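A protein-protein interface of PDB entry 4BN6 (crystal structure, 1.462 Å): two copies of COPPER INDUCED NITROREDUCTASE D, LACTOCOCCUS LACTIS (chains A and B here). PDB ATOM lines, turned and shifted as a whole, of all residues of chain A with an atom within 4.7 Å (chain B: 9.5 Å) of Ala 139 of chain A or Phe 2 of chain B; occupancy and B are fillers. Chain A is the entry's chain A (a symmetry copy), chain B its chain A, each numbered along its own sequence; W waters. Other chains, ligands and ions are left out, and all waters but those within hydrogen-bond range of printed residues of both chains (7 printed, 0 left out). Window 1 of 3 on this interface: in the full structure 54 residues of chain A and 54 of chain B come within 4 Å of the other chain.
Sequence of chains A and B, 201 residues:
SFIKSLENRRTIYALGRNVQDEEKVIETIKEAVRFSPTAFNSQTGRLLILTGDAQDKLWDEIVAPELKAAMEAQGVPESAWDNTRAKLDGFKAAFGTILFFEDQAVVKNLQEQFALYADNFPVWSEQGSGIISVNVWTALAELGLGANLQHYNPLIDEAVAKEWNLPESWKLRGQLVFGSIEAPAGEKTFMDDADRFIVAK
The side-chain carboxylate (OE2) of Glu 142 of chain A is in hydrogen-bond range of the backbone NH (N) of Phe 2 of chain B. The side-chain carboxylate of Glu 142 of chain B is in hydrogen-bond range of the backbone NH of Phe 2 of chain A, at 2.9 Å.
The backbone NH (N) of Lys 4 of chain B sits close to the side-chain hydroxyl (OG) of Ser 1 of chain B (3.1 Å). O of Ser 1 of chain B sits at hydrogen-bond distance from OG of Ser 5 of chain B (3.2 Å). The side-chain hydroxyl of Thr 138 of chain B is in hydrogen-bond range of the backbone carbonyl oxygen of Val 134 of chain B, 2.9 Å away.
Among the printed residues, merely in contact across the chains: Phe 2 of chain A with Phe 2 of chain B (3.6 Å), Phe 2 of chain A with Ser 5 of chain B (3.8 Å), Phe 2 of chain A with Asn 135 of chain B (3.4 Å), Phe 2 of chain A with Thr 138 of chain B (3.4 Å), Phe 2 of chain A with Ala 139 of chain B (3.6 Å), Ser 5 of chain A with Phe 2 of chain B (3.8 Å), Leu 6 of chain A with Asn 135 of chain B (3.6 Å), Thr 28 of chain A with Ile 3 of chain B (3.9 Å), Ala 32 of chain A with Ile 3 of chain B (3.8 Å), Ala 32 of chain A with Leu 6 of chain B (3.9 Å), Asn 135 of chain A with Phe 2 of chain B (3.4 Å), Asn 135 of chain A with Leu 6 of chain B (3.6 Å), Thr 138 of chain A with Phe 2 of chain B (3.4 Å), Ala 139 of chain A with Phe 2 of chain B (3.6 Å) and Glu 142 of chain A with Ser 1 of chain B (3.7 Å).
Of the printed residues of chain B, Thr 28 of chain A touches Ile 3. Thr 138 of chain A touches one residue of chain B. Of the printed residues of chain B, Ala 139 of chain A touches Phe 2 (3.6 Å). Phe 2 of chain B touches six residues of chain A. Of the printed residues of chain A, Glu 142 of chain B touches Phe 2. The nearest residue of chain B that does not touch Ala 139 of chain A is Ile 3 of chain B (4.2 Å).
Printed residues of chain B that touch a printed residue of chain A: Ser 1, Phe 2, Ile 3, Ser 5, Leu 6, Asn 135, Thr 138, Ala 139 and Glu 142. Hydrophobic or aromatic side chains of chain B that line the printed part of chain A: Phe 2, Ile 3, Leu 6 and Ala 139. Among the printed residues, 17 pairs touch across the chains.
Phe 2 of chain A touches Ser 5 of chain B, and with the chains exchanged Ser 5 of chain A touches Phe 2 of chain B. Phe 2 of chain A touches Thr 138 of chain B, and with the chains exchanged Thr 138 of chain A touches Phe 2 of chain B. Phe 2 of chain A touches Glu 142 of chain B, and with the chains exchanged Glu 142 of chain A touches Phe 2 of chain B. Leu 6 of chain A touches Asn 135 of chain B, and with the chains exchanged Asn 135 of chain A touches Leu 6 of chain B. Of the 17 pairs that touch across the chains among the printed residues, 13 have their exchanged pair printed and touching as well.
Water W5 lies within hydrogen-bond range of OE1 of Glu 142 of chain A (2.6 Å), OG of Ser 1 of chain B (2.6 Å), N of Ile 3 of chain B (3.0 Å) and N of Phe 2 of chain B (3.2 Å). Water W2 lies within hydrogen-bond range of OD1 of Asn 135 of chain A (2.8 Å), OD1 of Asn 135 of chain B (2.9 Å) and OG1 of Thr 138 of chain A (3.4 Å). Water W4 lies within hydrogen-bond range of the side-chain amide oxygen of Asn 135 of chain B (2.8 Å), the side-chain amide oxygen of Asn 135 of chain A (2.9 Å) and the side-chain hydroxyl of Thr 138 of chain B (3.4 Å). Water W7 lies within hydrogen-bond range of ND2 of Asn 135 of chain B and OG1 of Thr 138 of chain A. Water W3 lies within hydrogen-bond range of ND2 of Asn 135 of chain A (3.0 Å) and OG1 of Thr 138 of chain B (3.3 Å). Water W1 lies within hydrogen-bond range of the side-chain hydroxyl of Ser 5 of chain A and the side-chain hydroxyl of Ser 5 of chain B.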
ATOM      1  N   PHE A   2      -7.468   1.629   6.948  1.00  0.00           N
ATOM      2  CA  PHE A   2      -6.303   1.123   7.651  1.00  0.00           C
ATOM      3  C   PHE A   2      -5.695   2.182   8.579  1.00  0.00           C
ATOM      4  O   PHE A   2      -5.315   1.877   9.701  1.00  0.00           O
ATOM      5  CB  PHE A   2      -5.246   0.640   6.652  1.00  0.00           C
ATOM      6  CG  PHE A   2      -3.981   0.169   7.301  1.00  0.00           C
ATOM      7  CD1 PHE A   2      -3.952  -1.029   8.001  1.00  0.00           C
ATOM      8  CD2 PHE A   2      -2.823   0.922   7.221  1.00  0.00           C
ATOM      9  CE1 PHE A   2      -2.788  -1.452   8.613  1.00  0.00           C
ATOM     10  CE2 PHE A   2      -1.658   0.497   7.836  1.00  0.00           C
ATOM     11  CZ  PHE A   2      -1.650  -0.700   8.529  1.00  0.00           C
ATOM     12  N   SER A   5      -7.674   2.388  11.623  1.00  0.00           N
ATOM     13  CA  SER A   5      -7.409   1.232  12.464  1.00  0.00           C
ATOM     14  C   SER A   5      -6.149   1.470  13.281  1.00  0.00           C
ATOM     15  O   SER A   5      -6.111   1.180  14.472  1.00  0.00           O
ATOM     16  CB  SER A   5      -7.272  -0.051  11.634  1.00  0.00           C
ATOM     17  OG  SER A   5      -8.501  -0.367  11.006  1.00  0.00           O
ATOM     18  N   LEU A   6      -5.116   2.016  12.649  1.00  0.00           N
ATOM     19  CA  LEU A   6      -3.891   2.334  13.372  1.00  0.00           C
ATOM     20  C   LEU A   6      -4.151   3.360  14.471  1.00  0.00           C
ATOM     21  O   LEU A   6      -3.660   3.208  15.591  1.00  0.00           O
ATOM     22  CB  LEU A   6      -2.820   2.874  12.425  1.00  0.00           C
ATOM     23  CG  LEU A   6      -2.233   1.902  11.406  1.00  0.00           C
ATOM     24  CD1 LEU A   6      -1.098   2.579  10.671  1.00  0.00           C
ATOM     25  CD2 LEU A   6      -1.748   0.612  12.056  1.00  0.00           C
ATOM     26  N   THR A  28      -8.435 -13.976  15.883  1.00  0.00           N
ATOM     27  CA  THR A  28      -7.897 -12.747  15.343  1.00  0.00           C
ATOM     28  C   THR A  28      -6.425 -12.582  15.710  1.00  0.00           C
ATOM     29  O   THR A  28      -5.632 -12.076  14.912  1.00  0.00           O
ATOM     30  CB  THR A  28      -8.727 -11.525  15.777  1.00  0.00           C
ATOM     31  OG1 THR A  28     -10.117 -11.793  15.567  1.00  0.00           O
ATOM     32  CG2 THR A  28      -8.367 -10.337  14.932  1.00  0.00           C
ATOM     33  N   ALA A  32      -3.527 -12.170  12.865  1.00  0.00           N
ATOM     34  CA  ALA A  32      -2.666 -11.003  12.829  1.00  0.00           C
ATOM     35  C   ALA A  32      -1.204 -11.425  12.730  1.00  0.00           C
ATOM     36  O   ALA A  32      -0.423 -10.797  12.011  1.00  0.00           O
ATOM     37  CB  ALA A  32      -2.896 -10.117  14.052  1.00  0.00           C
ATOM     38  N   ASN A 135       0.696  -5.686  15.282  1.00  0.00           N
ATOM     39  CA  ASN A 135      -0.395  -6.169  14.456  1.00  0.00           C
ATOM     40  C   ASN A 135      -1.458  -6.846  15.324  1.00  0.00           C
ATOM     41  O   ASN A 135      -2.652  -6.629  15.138  1.00  0.00           O
ATOM     42  CB  ASN A 135       0.095  -7.076  13.321  1.00  0.00           C
ATOM     43  CG  ASN A 135       0.645  -6.289  12.149  1.00  0.00           C
ATOM     44  OD1 ASN A 135       0.392  -5.090  12.019  1.00  0.00           O
ATOM     45  ND2 ASN A 135       1.403  -6.959  11.289  1.00  0.00           N
ATOM     46  N   VAL A 136      -1.031  -7.640  16.296  1.00  0.00           N
ATOM     47  CA  VAL A 136      -1.985  -8.232  17.225  1.00  0.00           C
ATOM     48  C   VAL A 136      -2.693  -7.143  18.054  1.00  0.00           C
ATOM     49  O   VAL A 136      -3.912  -7.158  18.215  1.00  0.00           O
ATOM     50  CB  VAL A 136      -1.299  -9.238  18.158  1.00  0.00           C
ATOM     51  CG1 VAL A 136      -2.234  -9.644  19.295  1.00  0.00           C
ATOM     52  CG2 VAL A 136      -0.840 -10.448  17.371  1.00  0.00           C
ATOM     53  N   TRP A 137      -1.920  -6.201  18.576  1.00  0.00           N
ATOM     54  CA  TRP A 137      -2.457  -5.088  19.364  1.00  0.00           C
ATOM     55  C   TRP A 137      -3.543  -4.327  18.590  1.00  0.00           C
ATOM     56  O   TRP A 137      -4.619  -4.028  19.117  1.00  0.00           O
ATOM     57  CB  TRP A 137      -1.281  -4.180  19.712  1.00  0.00           C
ATOM     58  CG  TRP A 137      -1.434  -3.177  20.820  1.00  0.00           C
ATOM     59  CD1 TRP A 137      -2.569  -2.772  21.455  1.00  0.00           C
ATOM     60  CD2 TRP A 137      -0.362  -2.449  21.397  1.00  0.00           C
ATOM     61  NE1 TRP A 137      -2.256  -1.816  22.409  1.00  0.00           N
ATOM     62  CE2 TRP A 137      -0.901  -1.612  22.391  1.00  0.00           C
ATOM     63  CE3 TRP A 137       1.016  -2.423  21.166  1.00  0.00           C
ATOM     64  CZ2 TRP A 137      -0.105  -0.758  23.144  1.00  0.00           C
ATOM     65  CZ3 TRP A 137       1.800  -1.586  21.916  1.00  0.00           C
ATOM     66  CH2 TRP A 137       1.240  -0.765  22.898  1.00  0.00           C
ATOM     67  N   THR A 138      -3.268  -4.031  17.326  1.00  0.00           N
ATOM     68  CA  THR A 138      -4.210  -3.286  16.501  1.00  0.00           C
ATOM     69  C   THR A 138      -5.448  -4.122  16.169  1.00  0.00           C
ATOM     70  O   THR A 138      -6.568  -3.623  16.163  1.00  0.00           O
ATOM     71  CB  THR A 138      -3.525  -2.775  15.224  1.00  0.00           C
ATOM     72  OG1 THR A 138      -2.387  -1.978  15.584  1.00  0.00           O
ATOM     73  CG2 THR A 138      -4.484  -1.928  14.401  1.00  0.00           C
ATOM     74  N   ALA A 139      -5.248  -5.405  15.904  1.00  0.00           N
ATOM     75  CA  ALA A 139      -6.357  -6.302  15.638  1.00  0.00           C
ATOM     76  C   ALA A 139      -7.307  -6.398  16.837  1.00  0.00           C
ATOM     77  O   ALA A 139      -8.530  -6.420  16.679  1.00  0.00           O
ATOM     78  CB  ALA A 139      -5.830  -7.679  15.254  1.00  0.00           C
ATOM     79  N   LEU A 140      -6.738  -6.453  18.033  1.00  0.00           N
ATOM     80  CA  LEU A 140      -7.541  -6.477  19.250  1.00  0.00           C
ATOM     81  C   LEU A 140      -8.328  -5.180  19.388  1.00  0.00           C
ATOM     82  O   LEU A 140      -9.501  -5.200  19.755  1.00  0.00           O
ATOM     83  CB  LEU A 140      -6.653  -6.685  20.473  1.00  0.00           C
ATOM     84  CG  LEU A 140      -6.018  -8.075  20.588  1.00  0.00           C
ATOM     85  CD1 LEU A 140      -5.017  -8.093  21.713  1.00  0.00           C
ATOM     86  CD2 LEU A 140      -7.082  -9.144  20.812  1.00  0.00           C
ATOM     87  N   ALA A 141      -7.684  -4.057  19.090  1.00  0.00           N
ATOM     88  CA  ALA A 141      -8.366  -2.770  19.168  1.00  0.00           C
ATOM     89  C   ALA A 141      -9.547  -2.706  18.205  1.00  0.00           C
ATOM     90  O   ALA A 141     -10.569  -2.080  18.509  1.00  0.00           O
ATOM     91  CB  ALA A 141      -7.397  -1.623  18.909  1.00  0.00           C
ATOM     92  N   GLU A 142      -9.424  -3.354  17.043  1.00  0.00           N
ATOM     93  CA  GLU A 142     -10.530  -3.376  16.097  1.00  0.00           C
ATOM     94  C   GLU A 142     -11.750  -4.109  16.661  1.00  0.00           C
ATOM     95  O   GLU A 142     -12.891  -3.794  16.319  1.00  0.00           O
ATOM     96  CB  GLU A 142     -10.113  -4.008  14.759  1.00  0.00           C
ATOM     97  CG  GLU A 142     -11.266  -4.012  13.770  1.00  0.00           C
ATOM     98  CD  GLU A 142     -10.947  -4.712  12.466  1.00  0.00           C
ATOM     99  OE1 GLU A 142     -10.560  -5.898  12.494  1.00  0.00           O
ATOM    100  OE2 GLU A 142     -11.092  -4.067  11.407  1.00  0.00           O
ATOM    101  N   LEU A 143     -11.506  -5.084  17.533  1.00  0.00           N
ATOM    102  CA  LEU A 143     -12.580  -5.809  18.214  1.00  0.00           C
ATOM    103  C   LEU A 143     -13.144  -5.032  19.399  1.00  0.00           C
ATOM    104  O   LEU A 143     -14.076  -5.496  20.056  1.00  0.00           O
ATOM    105  CB  LEU A 143     -12.088  -7.169  18.718  1.00  0.00           C
ATOM    106  CG  LEU A 143     -11.616  -8.172  17.663  1.00  0.00           C
ATOM    107  CD1 LEU A 143     -11.224  -9.476  18.340  1.00  0.00           C
ATOM    108  CD2 LEU A 143     -12.683  -8.394  16.616  1.00  0.00           C
ATOM    109  N   SER B   1     -11.902  -4.195   7.121  1.00  0.00           N
ATOM    110  CA  SER B   1     -11.305  -5.260   7.913  1.00  0.00           C
ATOM    111  C   SER B   1      -9.806  -5.037   8.058  1.00  0.00           C
ATOM    112  O   SER B   1      -9.079  -5.021   7.079  1.00  0.00           O
ATOM    113  CB  SER B   1     -11.572  -6.627   7.267  1.00  0.00           C
ATOM    114  OG  SER B   1     -10.869  -7.681   7.920  1.00  0.00           O
ATOM    115  N   PHE B   2      -9.349  -4.872   9.292  1.00  0.00           N
ATOM    116  CA  PHE B   2      -7.925  -4.766   9.557  1.00  0.00           C
ATOM    117  C   PHE B   2      -7.174  -6.035   9.136  1.00  0.00           C
ATOM    118  O   PHE B   2      -6.099  -5.956   8.559  1.00  0.00           O
ATOM    119  CB  PHE B   2      -7.679  -4.485  11.043  1.00  0.00           C
ATOM    120  CG  PHE B   2      -6.228  -4.434  11.410  1.00  0.00           C
ATOM    121  CD1 PHE B   2      -5.439  -3.362  11.015  1.00  0.00           C
ATOM    122  CD2 PHE B   2      -5.646  -5.455  12.139  1.00  0.00           C
ATOM    123  CE1 PHE B   2      -4.096  -3.326  11.340  1.00  0.00           C
ATOM    124  CE2 PHE B   2      -4.301  -5.418  12.462  1.00  0.00           C
ATOM    125  CZ  PHE B   2      -3.532  -4.341  12.060  1.00  0.00           C
ATOM    126  N   ILE B   3      -7.725  -7.203   9.440  1.00  0.00           N
ATOM    127  CA  ILE B   3      -7.064  -8.448   9.056  1.00  0.00           C
ATOM    128  C   ILE B   3      -6.932  -8.536   7.536  1.00  0.00           C
ATOM    129  O   ILE B   3      -5.885  -8.924   7.035  1.00  0.00           O
ATOM    130  CB  ILE B   3      -7.794  -9.688   9.626  1.00  0.00           C
ATOM    131  CG1 ILE B   3      -7.683  -9.723  11.155  1.00  0.00           C
ATOM    132  CG2 ILE B   3      -7.224 -10.974   9.036  1.00  0.00           C
ATOM    133  CD1 ILE B   3      -6.248  -9.761  11.686  1.00  0.00           C
ATOM    134  N   LYS B   4      -7.976  -8.149   6.811  1.00  0.00           N
ATOM    135  CA  LYS B   4      -7.917  -8.120   5.351  1.00  0.00           C
ATOM    136  C   LYS B   4      -6.828  -7.161   4.873  1.00  0.00           C
ATOM    137  O   LYS B   4      -6.112  -7.456   3.922  1.00  0.00           O
ATOM    138  CB  LYS B   4      -9.270  -7.707   4.770  1.00  0.00           C
ATOM    139  CG  LYS B   4     -10.422  -8.606   5.156  1.00  0.00           C
ATOM    140  CD  LYS B   4     -10.366  -9.961   4.484  1.00  0.00           C
ATOM    141  CE  LYS B   4     -11.542 -10.817   4.927  1.00  0.00           C
ATOM    142  NZ  LYS B   4     -12.845 -10.221   4.510  1.00  0.00           N
ATOM    143  N   SER B   5      -6.697  -6.009   5.532  1.00  0.00           N
ATOM    144  CA  SER B   5      -5.658  -5.054   5.178  1.00  0.00           C
ATOM    145  C   SER B   5      -4.291  -5.699   5.342  1.00  0.00           C
ATOM    146  O   SER B   5      -3.421  -5.549   4.491  1.00  0.00           O
ATOM    147  CB  SER B   5      -5.751  -3.778   6.024  1.00  0.00           C
ATOM    148  OG  SER B   5      -6.955  -3.086   5.744  1.00  0.00           O
ATOM    149  N   LEU B   6      -4.099  -6.434   6.433  1.00  0.00           N
ATOM    150  CA  LEU B   6      -2.839  -7.137   6.638  1.00  0.00           C
ATOM    151  C   LEU B   6      -2.592  -8.160   5.534  1.00  0.00           C
ATOM    152  O   LEU B   6      -1.479  -8.256   5.013  1.00  0.00           O
ATOM    153  CB  LEU B   6      -2.820  -7.844   7.992  1.00  0.00           C
ATOM    154  CG  LEU B   6      -2.795  -6.968   9.240  1.00  0.00           C
ATOM    155  CD1 LEU B   6      -2.631  -7.845  10.461  1.00  0.00           C
ATOM    156  CD2 LEU B   6      -1.686  -5.924   9.186  1.00  0.00           C
ATOM    157  N   GLU B   7      -3.619  -8.928   5.188  1.00  0.00           N
ATOM    158  CA  GLU B   7      -3.472  -9.970   4.181  1.00  0.00           C
ATOM    159  C   GLU B   7      -3.121  -9.368   2.823  1.00  0.00           C
ATOM    160  O   GLU B   7      -2.387  -9.982   2.041  1.00  0.00           O
ATOM    161  CB  GLU B   7      -4.748 -10.813   4.067  1.00  0.00           C
ATOM    162  CG  GLU B   7      -4.588 -12.016   3.143  1.00  0.00           C
ATOM    163  CD  GLU B   7      -5.764 -12.972   3.186  1.00  0.00           C
ATOM    164  OE1 GLU B   7      -6.808 -12.624   3.774  1.00  0.00           O
ATOM    165  OE2 GLU B   7      -5.639 -14.080   2.627  1.00  0.00           O
ATOM    166  N   ASN B   8      -3.652  -8.179   2.550  1.00  0.00           N
ATOM    167  CA  ASN B   8      -3.445  -7.507   1.264  1.00  0.00           C
ATOM    168  C   ASN B   8      -2.020  -7.025   1.035  1.00  0.00           C
ATOM    169  O   ASN B   8      -1.603  -6.825  -0.105  1.00  0.00           O
ATOM    170  CB  ASN B   8      -4.411  -6.332   1.094  1.00  0.00           C
ATOM    171  CG  ASN B   8      -5.822  -6.777   0.779  1.00  0.00           C
ATOM    172  OD1 ASN B   8      -6.046  -7.909   0.355  1.00  0.00           O
ATOM    173  ND2 ASN B   8      -6.786  -5.883   0.985  1.00  0.00           N
ATOM    174  N   ARG B   9      -1.277  -6.805   2.113  1.00  0.00           N
ATOM    175  CA  ARG B   9       0.114  -6.378   2.013  1.00  0.00           C
ATOM    176  C   ARG B   9       0.979  -7.567   1.622  1.00  0.00           C
ATOM    177  O   ARG B   9       0.956  -8.602   2.285  1.00  0.00           O
ATOM    178  CB  ARG B   9       0.622  -5.807   3.338  1.00  0.00           C
ATOM    179  CG  ARG B   9       2.068  -5.285   3.284  1.00  0.00           C
ATOM    180  CD  ARG B   9       2.874  -5.646   4.523  1.00  0.00           C
ATOM    181  NE  ARG B   9       2.756  -7.069   4.807  1.00  0.00           N
ATOM    182  CZ  ARG B   9       3.450  -8.029   4.210  1.00  0.00           C
ATOM    183  NH1 ARG B   9       4.389  -7.740   3.314  1.00  0.00           N
ATOM    184  NH2 ARG B   9       3.214  -9.293   4.523  1.00  0.00           N
ATOM    185  N   VAL B 134       6.388  -1.817   8.465  1.00  0.00           N
ATOM    186  CA  VAL B 134       5.253  -2.618   8.009  1.00  0.00           C
ATOM    187  C   VAL B 134       3.954  -1.820   8.018  1.00  0.00           C
ATOM    188  O   VAL B 134       3.081  -2.058   7.182  1.00  0.00           O
ATOM    189  CB  VAL B 134       5.063  -3.942   8.804  1.00  0.00           C
ATOM    190  CG1 VAL B 134       6.313  -4.798   8.707  1.00  0.00           C
ATOM    191  CG2 VAL B 134       4.663  -3.679  10.259  1.00  0.00           C
ATOM    192  N   ASN B 135       3.817  -0.854   8.929  1.00  0.00           N
ATOM    193  CA  ASN B 135       2.630  -0.020   8.904  1.00  0.00           C
ATOM    194  C   ASN B 135       2.604   0.826   7.629  1.00  0.00           C
ATOM    195  O   ASN B 135       1.568   0.954   6.982  1.00  0.00           O
ATOM    196  CB  ASN B 135       2.494   0.833  10.172  1.00  0.00           C
ATOM    197  CG  ASN B 135       1.929   0.049  11.337  1.00  0.00           C
ATOM    198  OD1 ASN B 135       1.344  -1.021  11.155  1.00  0.00           O
ATOM    199  ND2 ASN B 135       2.098   0.575  12.544  1.00  0.00           N
ATOM    200  N   THR B 138       1.840  -1.591   4.665  1.00  0.00           N
ATOM    201  CA  THR B 138       0.435  -1.973   4.613  1.00  0.00           C
ATOM    202  C   THR B 138      -0.446  -0.809   4.153  1.00  0.00           C
ATOM    203  O   THR B 138      -1.388  -0.990   3.389  1.00  0.00           O
ATOM    204  CB  THR B 138      -0.029  -2.518   5.973  1.00  0.00           C
ATOM    205  OG1 THR B 138       0.809  -3.621   6.351  1.00  0.00           O
ATOM    206  CG2 THR B 138      -1.471  -2.994   5.899  1.00  0.00           C
ATOM    207  N   ALA B 139      -0.132   0.394   4.611  1.00  0.00           N
ATOM    208  CA  ALA B 139      -0.861   1.575   4.190  1.00  0.00           C
ATOM    209  C   ALA B 139      -0.749   1.800   2.677  1.00  0.00           C
ATOM    210  O   ALA B 139      -1.723   2.162   2.015  1.00  0.00           O
ATOM    211  CB  ALA B 139      -0.363   2.794   4.957  1.00  0.00           C
ATOM    212  N   GLU B 142      -2.947  -0.576   0.859  1.00  0.00           N
ATOM    213  CA  GLU B 142      -4.344  -0.167   0.870  1.00  0.00           C
ATOM    214  C   GLU B 142      -4.664   0.804  -0.270  1.00  0.00           C
ATOM    215  O   GLU B 142      -5.787   0.839  -0.774  1.00  0.00           O
ATOM    216  CB  GLU B 142      -4.736   0.461   2.217  1.00  0.00           C
ATOM    217  CG  GLU B 142      -6.198   0.870   2.229  1.00  0.00           C
ATOM    218  CD  GLU B 142      -6.621   1.585   3.495  1.00  0.00           C
ATOM    219  OE1 GLU B 142      -6.010   2.617   3.839  1.00  0.00           O
ATOM    220  OE2 GLU B 142      -7.577   1.111   4.141  1.00  0.00           O
HETATM  221  O   HOH W   1      -8.407  -1.622   8.121  1.00  0.00           O
HETATM  222  O   HOH W   2      -0.250  -2.509  13.025  1.00  0.00           O
HETATM  223  O   HOH W   3       1.959  -5.828   8.547  1.00  0.00           O
HETATM  224  O   HOH W   4       0.843  -3.427   9.722  1.00  0.00           O
HETATM  225  O   HOH W   5     -10.486  -7.627  10.522  1.00  0.00           O
HETATM  226  O   HOH W   6      -6.763   4.451   5.557  1.00  0.00           O
HETATM  227  O   HOH W   7       0.437  -0.385  14.874  1.00  0.00           O
